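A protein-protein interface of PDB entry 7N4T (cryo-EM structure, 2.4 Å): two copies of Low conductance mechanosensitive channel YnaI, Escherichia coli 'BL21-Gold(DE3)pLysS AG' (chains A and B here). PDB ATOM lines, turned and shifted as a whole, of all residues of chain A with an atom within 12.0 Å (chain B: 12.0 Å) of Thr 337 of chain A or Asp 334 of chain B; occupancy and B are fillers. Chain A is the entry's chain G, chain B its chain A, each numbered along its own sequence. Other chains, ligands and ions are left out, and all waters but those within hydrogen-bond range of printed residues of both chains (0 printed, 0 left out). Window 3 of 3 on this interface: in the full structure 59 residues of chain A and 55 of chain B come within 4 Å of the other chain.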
ATOM      1  N   LEU A 331     -35.843 -12.240  -9.296  1.00  0.00           N
ATOM      2  CA  LEU A 331     -35.122 -12.124  -8.018  1.00  0.00           C
ATOM      3  C   LEU A 331     -33.918 -11.155  -7.788  1.00  0.00           C
ATOM      4  O   LEU A 331     -33.820 -10.587  -6.699  1.00  0.00           O
ATOM      5  CB  LEU A 331     -34.850 -13.541  -7.485  1.00  0.00           C
ATOM      6  CG  LEU A 331     -36.092 -14.207  -6.831  1.00  0.00           C
ATOM      7  CD1 LEU A 331     -35.787 -15.482  -6.062  1.00  0.00           C
ATOM      8  CD2 LEU A 331     -36.899 -13.282  -5.929  1.00  0.00           C
ATOM      9  N   TYR A 332     -33.012 -10.974  -8.757  1.00  0.00           N
ATOM     10  CA  TYR A 332     -31.860 -10.040  -8.603  1.00  0.00           C
ATOM     11  C   TYR A 332     -31.062 -10.132  -7.275  1.00  0.00           C
ATOM     12  O   TYR A 332     -30.930  -9.132  -6.568  1.00  0.00           O
ATOM     13  CB  TYR A 332     -32.318  -8.575  -8.706  1.00  0.00           C
ATOM     14  CG  TYR A 332     -32.766  -8.160 -10.087  1.00  0.00           C
ATOM     15  CD1 TYR A 332     -31.968  -8.398 -11.198  1.00  0.00           C
ATOM     16  CD2 TYR A 332     -33.983  -7.522 -10.278  1.00  0.00           C
ATOM     17  CE1 TYR A 332     -32.374  -8.016 -12.463  1.00  0.00           C
ATOM     18  CE2 TYR A 332     -34.398  -7.137 -11.539  1.00  0.00           C
ATOM     19  CZ  TYR A 332     -33.590  -7.385 -12.627  1.00  0.00           C
ATOM     20  OH  TYR A 332     -34.000  -7.003 -13.883  1.00  0.00           O
ATOM     21  N   MET A 333     -30.540 -11.313  -6.940  1.00  0.00           N
ATOM     22  CA  MET A 333     -29.783 -11.468  -5.657  1.00  0.00           C
ATOM     23  C   MET A 333     -28.447 -10.753  -5.524  1.00  0.00           C
ATOM     24  O   MET A 333     -27.657 -10.770  -6.461  1.00  0.00           O
ATOM     25  CB  MET A 333     -29.430 -12.938  -5.471  1.00  0.00           C
ATOM     26  CG  MET A 333     -30.613 -13.806  -5.214  1.00  0.00           C
ATOM     27  SD  MET A 333     -30.002 -15.485  -5.114  1.00  0.00           S
ATOM     28  CE  MET A 333     -31.602 -16.212  -4.877  1.00  0.00           C
ATOM     29  N   ASP A 334     -28.155 -10.183  -4.354  1.00  0.00           N
ATOM     30  CA  ASP A 334     -26.921  -9.451  -4.123  1.00  0.00           C
ATOM     31  C   ASP A 334     -26.451 -10.041  -2.800  1.00  0.00           C
ATOM     32  O   ASP A 334     -26.868  -9.576  -1.753  1.00  0.00           O
ATOM     33  CB  ASP A 334     -27.295  -7.978  -3.953  1.00  0.00           C
ATOM     34  CG  ASP A 334     -26.132  -7.132  -3.472  1.00  0.00           C
ATOM     35  OD1 ASP A 334     -25.899  -6.053  -4.057  1.00  0.00           O
ATOM     36  OD2 ASP A 334     -25.450  -7.545  -2.511  1.00  0.00           O
ATOM     37  N   ASN A 335     -25.665 -11.114  -2.845  1.00  0.00           N
ATOM     38  CA  ASN A 335     -25.190 -11.773  -1.626  1.00  0.00           C
ATOM     39  C   ASN A 335     -24.482 -10.931  -0.558  1.00  0.00           C
ATOM     40  O   ASN A 335     -23.477 -10.287  -0.860  1.00  0.00           O
ATOM     41  CB  ASN A 335     -24.379 -13.037  -1.943  1.00  0.00           C
ATOM     42  CG  ASN A 335     -24.606 -14.144  -0.932  1.00  0.00           C
ATOM     43  OD1 ASN A 335     -25.033 -13.895   0.195  1.00  0.00           O
ATOM     44  ND2 ASN A 335     -24.310 -15.377  -1.329  1.00  0.00           N
ATOM     45  N   ILE A 336     -24.989 -10.916   0.696  1.00  0.00           N
ATOM     46  CA  ILE A 336     -24.377 -10.054   1.702  1.00  0.00           C
ATOM     47  C   ILE A 336     -24.030 -10.867   2.944  1.00  0.00           C
ATOM     48  O   ILE A 336     -23.857 -10.309   4.034  1.00  0.00           O
ATOM     49  CB  ILE A 336     -25.297  -8.867   2.054  1.00  0.00           C
ATOM     50  CG1 ILE A 336     -26.580  -9.342   2.748  1.00  0.00           C
ATOM     51  CG2 ILE A 336     -25.643  -8.079   0.801  1.00  0.00           C
ATOM     52  CD1 ILE A 336     -27.292  -8.258   3.523  1.00  0.00           C
ATOM     53  N   THR A 337     -23.927 -12.184   2.793  1.00  0.00           N
ATOM     54  CA  THR A 337     -23.554 -13.025   3.917  1.00  0.00           C
ATOM     55  C   THR A 337     -22.106 -12.744   4.320  1.00  0.00           C
ATOM     56  O   THR A 337     -21.280 -12.383   3.476  1.00  0.00           O
ATOM     57  CB  THR A 337     -23.718 -14.501   3.564  1.00  0.00           C
ATOM     58  OG1 THR A 337     -23.638 -15.294   4.754  1.00  0.00           O
ATOM     59  CG2 THR A 337     -22.635 -14.945   2.590  1.00  0.00           C
ATOM     60  N   PRO A 338     -21.770 -12.893   5.599  1.00  0.00           N
ATOM     61  CA  PRO A 338     -20.393 -12.629   6.036  1.00  0.00           C
ATOM     62  C   PRO A 338     -19.408 -13.514   5.292  1.00  0.00           C
ATOM     63  O   PRO A 338     -19.694 -14.694   5.040  1.00  0.00           O
ATOM     64  CB  PRO A 338     -20.423 -12.965   7.535  1.00  0.00           C
ATOM     65  CG  PRO A 338     -21.847 -12.841   7.928  1.00  0.00           C
ATOM     66  CD  PRO A 338     -22.641 -13.258   6.731  1.00  0.00           C
ATOM     67  N   PRO A 339     -18.231 -12.984   4.917  1.00  0.00           N
ATOM     68  CA  PRO A 339     -17.240 -13.821   4.228  1.00  0.00           C
ATOM     69  C   PRO A 339     -16.804 -15.024   5.058  1.00  0.00           C
ATOM     70  O   PRO A 339     -16.750 -14.915   6.284  1.00  0.00           O
ATOM     71  CB  PRO A 339     -16.065 -12.863   4.000  1.00  0.00           C
ATOM     72  CG  PRO A 339     -16.661 -11.504   4.041  1.00  0.00           C
ATOM     73  CD  PRO A 339     -17.787 -11.582   5.022  1.00  0.00           C
ATOM     74  N   THR B 330     -35.205  -7.239  -4.938  1.00  0.00           N
ATOM     75  CA  THR B 330     -33.859  -7.581  -4.494  1.00  0.00           C
ATOM     76  C   THR B 330     -33.948  -8.344  -3.178  1.00  0.00           C
ATOM     77  O   THR B 330     -34.934  -8.224  -2.446  1.00  0.00           O
ATOM     78  CB  THR B 330     -33.000  -6.325  -4.320  1.00  0.00           C
ATOM     79  OG1 THR B 330     -33.164  -5.471  -5.459  1.00  0.00           O
ATOM     80  CG2 THR B 330     -31.533  -6.692  -4.182  1.00  0.00           C
ATOM     81  N   LEU B 331     -32.918  -9.137  -2.873  1.00  0.00           N
ATOM     82  CA  LEU B 331     -33.042 -10.134  -1.817  1.00  0.00           C
ATOM     83  C   LEU B 331     -32.021 -10.030  -0.689  1.00  0.00           C
ATOM     84  O   LEU B 331     -32.361 -10.387   0.441  1.00  0.00           O
ATOM     85  CB  LEU B 331     -32.976 -11.546  -2.421  1.00  0.00           C
ATOM     86  CG  LEU B 331     -34.181 -11.952  -3.283  1.00  0.00           C
ATOM     87  CD1 LEU B 331     -34.186 -13.447  -3.536  1.00  0.00           C
ATOM     88  CD2 LEU B 331     -35.505 -11.528  -2.661  1.00  0.00           C
ATOM     89  N   TYR B 332     -30.796  -9.577  -0.939  1.00  0.00           N
ATOM     90  CA  TYR B 332     -29.811  -9.389   0.131  1.00  0.00           C
ATOM     91  C   TYR B 332     -29.703 -10.643   1.007  1.00  0.00           C
ATOM     92  O   TYR B 332     -30.088 -10.670   2.174  1.00  0.00           O
ATOM     93  CB  TYR B 332     -30.160  -8.165   0.983  1.00  0.00           C
ATOM     94  CG  TYR B 332     -30.168  -6.869   0.206  1.00  0.00           C
ATOM     95  CD1 TYR B 332     -29.016  -6.408  -0.415  1.00  0.00           C
ATOM     96  CD2 TYR B 332     -31.320  -6.105   0.097  1.00  0.00           C
ATOM     97  CE1 TYR B 332     -29.012  -5.226  -1.124  1.00  0.00           C
ATOM     98  CE2 TYR B 332     -31.323  -4.920  -0.612  1.00  0.00           C
ATOM     99  CZ  TYR B 332     -30.167  -4.486  -1.221  1.00  0.00           C
ATOM    100  OH  TYR B 332     -30.167  -3.307  -1.928  1.00  0.00           O
ATOM    101  N   MET B 333     -29.163 -11.691   0.383  1.00  0.00           N
ATOM    102  CA  MET B 333     -28.995 -13.008   0.999  1.00  0.00           C
ATOM    103  C   MET B 333     -28.091 -12.994   2.246  1.00  0.00           C
ATOM    104  O   MET B 333     -26.977 -12.495   2.189  1.00  0.00           O
ATOM    105  CB  MET B 333     -28.420 -13.984  -0.029  1.00  0.00           C
ATOM    106  CG  MET B 333     -29.374 -14.326  -1.163  1.00  0.00           C
ATOM    107  SD  MET B 333     -28.629 -15.408  -2.396  1.00  0.00           S
ATOM    108  CE  MET B 333     -28.559 -16.953  -1.493  1.00  0.00           C
ATOM    109  N   ASP B 334     -28.523 -13.647   3.324  1.00  0.00           N
ATOM    110  CA  ASP B 334     -27.790 -13.664   4.584  1.00  0.00           C
ATOM    111  C   ASP B 334     -27.229 -15.029   4.958  1.00  0.00           C
ATOM    112  O   ASP B 334     -26.119 -15.091   5.491  1.00  0.00           O
ATOM    113  CB  ASP B 334     -28.708 -13.180   5.715  1.00  0.00           C
ATOM    114  CG  ASP B 334     -27.932 -12.689   6.919  1.00  0.00           C
ATOM    115  OD1 ASP B 334     -26.965 -13.367   7.324  1.00  0.00           O
ATOM    116  OD2 ASP B 334     -28.278 -11.615   7.452  1.00  0.00           O
ATOM    117  N   ASN B 335     -27.951 -16.119   4.692  1.00  0.00           N
ATOM    118  CA  ASN B 335     -27.431 -17.478   4.862  1.00  0.00           C
ATOM    119  C   ASN B 335     -27.009 -17.735   6.314  1.00  0.00           C
ATOM    120  O   ASN B 335     -25.832 -17.907   6.634  1.00  0.00           O
ATOM    121  CB  ASN B 335     -26.263 -17.724   3.900  1.00  0.00           C
ATOM    122  CG  ASN B 335     -25.728 -19.138   3.984  1.00  0.00           C
ATOM    123  OD1 ASN B 335     -26.326 -20.002   4.621  1.00  0.00           O
ATOM    124  ND2 ASN B 335     -24.590 -19.379   3.343  1.00  0.00           N
ATOM    125  N   ILE B 336     -28.014 -17.753   7.192  1.00  0.00           N
ATOM    126  CA  ILE B 336     -27.780 -17.954   8.620  1.00  0.00           C
ATOM    127  C   ILE B 336     -27.856 -19.435   8.977  1.00  0.00           C
ATOM    128  O   ILE B 336     -27.987 -19.790  10.153  1.00  0.00           O
ATOM    129  CB  ILE B 336     -28.779 -17.145   9.471  1.00  0.00           C
ATOM    130  CG1 ILE B 336     -30.214 -17.637   9.255  1.00  0.00           C
ATOM    131  CG2 ILE B 336     -28.679 -15.667   9.139  1.00  0.00           C
ATOM    132  CD1 ILE B 336     -31.170 -17.223  10.351  1.00  0.00           C
ATOM    133  N   THR B 337     -27.782 -20.306   7.976  1.00  0.00           N
ATOM    134  CA  THR B 337     -27.873 -21.734   8.242  1.00  0.00           C
ATOM    135  C   THR B 337     -26.700 -22.173   9.119  1.00  0.00           C
ATOM    136  O   THR B 337     -25.578 -21.685   8.943  1.00  0.00           O
ATOM    137  CB  THR B 337     -27.870 -22.530   6.936  1.00  0.00           C
ATOM    138  OG1 THR B 337     -28.150 -23.909   7.210  1.00  0.00           O
ATOM    139  CG2 THR B 337     -26.518 -22.426   6.250  1.00  0.00           C
ATOM    140  N   PRO B 338     -26.917 -23.081  10.069  1.00  0.00           N
ATOM    141  CA  PRO B 338     -25.817 -23.518  10.939  1.00  0.00           C
ATOM    142  C   PRO B 338     -24.712 -24.175  10.131  1.00  0.00           C
ATOM    143  O   PRO B 338     -24.988 -24.872   9.144  1.00  0.00           O
ATOM    144  CB  PRO B 338     -26.489 -24.522  11.888  1.00  0.00           C
ATOM    145  CG  PRO B 338     -27.713 -24.969  11.175  1.00  0.00           C
ATOM    146  CD  PRO B 338     -28.172 -23.788  10.378  1.00  0.00           C
ATOM    147  N   PRO B 339     -23.438 -23.978  10.515  1.00  0.00           N
ATOM    148  CA  PRO B 339     -22.343 -24.627   9.785  1.00  0.00           C
ATOM    149  C   PRO B 339     -22.466 -26.148   9.761  1.00  0.00           C
ATOM    150  O   PRO B 339     -21.441 -26.830   9.735  1.00  0.00           O
ATOM    151  CB  PRO B 339     -21.094 -24.196  10.564  1.00  0.00           C
ATOM    152  CG  PRO B 339     -21.489 -22.951  11.268  1.00  0.00           C
ATOM    153  CD  PRO B 339     -22.938 -23.112  11.597  1.00  0.00           C
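OD1 of Asn 335 of chain A sits at hydrogen-bond distance from N of Thr 337 of chain A (3.3 Å).
Met 333 of chain A touches Leu 331 of chain B, but with the chains exchanged Leu 331 of chain A does not touch Met 333 of chain B (8.0 Å). Met 333 of chain B touches its own counterpart, Met 333 of chain A. Asp 334 of chain A touches Tyr 332 of chain B, but with the chains exchanged Tyr 332 of chain A does not touch Asp 334 of chain B (11.1 Å). Ile 336 of chain A touches Tyr 332 of chain B, but with the chains exchanged Tyr 332 of chain A does not touch Ile 336 of chain B (16.5 Å). 9 positions are printed for both chains. Of the 13 pairs that touch across the chains among the printed residues, 2 have their exchanged pair printed and touching as well.
Leu 331 of chain A touches Thr 330 of chain B (O to CA, 3.7 Å). Leu 331 of chain A touches Leu 331 of chain B. Thr 330 of chain B touches Tyr 332 of chain A. CD1 of Leu 331 of chain B touches CG of Met 333 of chain A (3.96 Å). O of Asp 334 of chain A touches CA of Tyr 332 of chain B (3.5 Å). Met 333 of chain B touches Asp 334 of chain A (N to O, 3.8 Å). Tyr 332 of chain B touches Ile 336 of chain A. OG1 of Thr 337 of chain A touches CB of Asn 335 of chain B, 3.7 Å away.
The side-chain amide oxygen of Asn 335 of chain A lies close to the backbone carbonyl oxygen of Met 333 of chain B (3.1 Å). O of Met 333 of chain B lies within hydrogen-bond range of N of Ile 336 of chain A (2.9 Å). The backbone carbonyl oxygen of Met 333 of chain B is in hydrogen-bond range of the backbone NH of Thr 337 of chain A, at 3.1 Å. The side-chain hydroxyl (OG1) of Thr 337 of chain A sits at hydrogen-bond distance from the backbone carbonyl oxygen (O) of Asp 334 of chain B, at 2.6 Å. The side-chain sulfur (SD) of Met 333 of chain A sits close to the side-chain sulfur (SD) of Met 333 of chain B, 3.0 Å away.
Printed residues of chain B within 4 Å of Leu 331 of chain A: Thr 330 and Leu 331. Printed residues of chain B within 4 Å of Met 333 of chain A: Leu 331 (3.96 Å) and Met 333 (3.0 Å). Of the printed residues of chain B, Asp 334 of chain A touches Tyr 332 and Met 333. Of chain B, only Met 333 (3.1 Å), Asp 334 (2.6 Å) and Asn 335 (3.7 Å) come within 4 Å of Thr 337 of chain A. No residue of chain B comes within 4 Å of Pro 338 of chain A. No residue of chain B comes within 4 Å of Pro 339 of chain A. Of the printed residues of chain A, Thr 330 of chain B touches Leu 331 and Tyr 332. Of the printed residues of chain A, Leu 331 of chain B touches Leu 331 and Met 333. Printed residues of chain A within 4 Å of Met 333 of chain B: Met 333, Asp 334, Asn 335, Ile 336 and Thr 337. Asn 335 of chain B touches one residue of chain A. No residue of chain A comes within 4 Å of Ile 336 of chain B. The nearest residue of chain A that does not touch Asp 334 of chain B is Pro 338 of chain A (4.1 Å).
Hydrophobic or aromatic side chains of chain B that line the printed part of chain A: Leu 331, Tyr 332 and Met 333. Along chain B the printed residues that touch a printed residue of chain A span positions 330 to 335. Of the 9 printed residues of chain A, 7 touch a printed residue of chain B. Hydrophobic or aromatic side chains of chain A within 4 Å of the printed part of chain B: Leu 331, Met 333 and Ile 336. Among the printed residues, no Asp or Glu carboxylate lies within 4 Å of a Lys or Arg side-chain nitrogen of the other chain.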
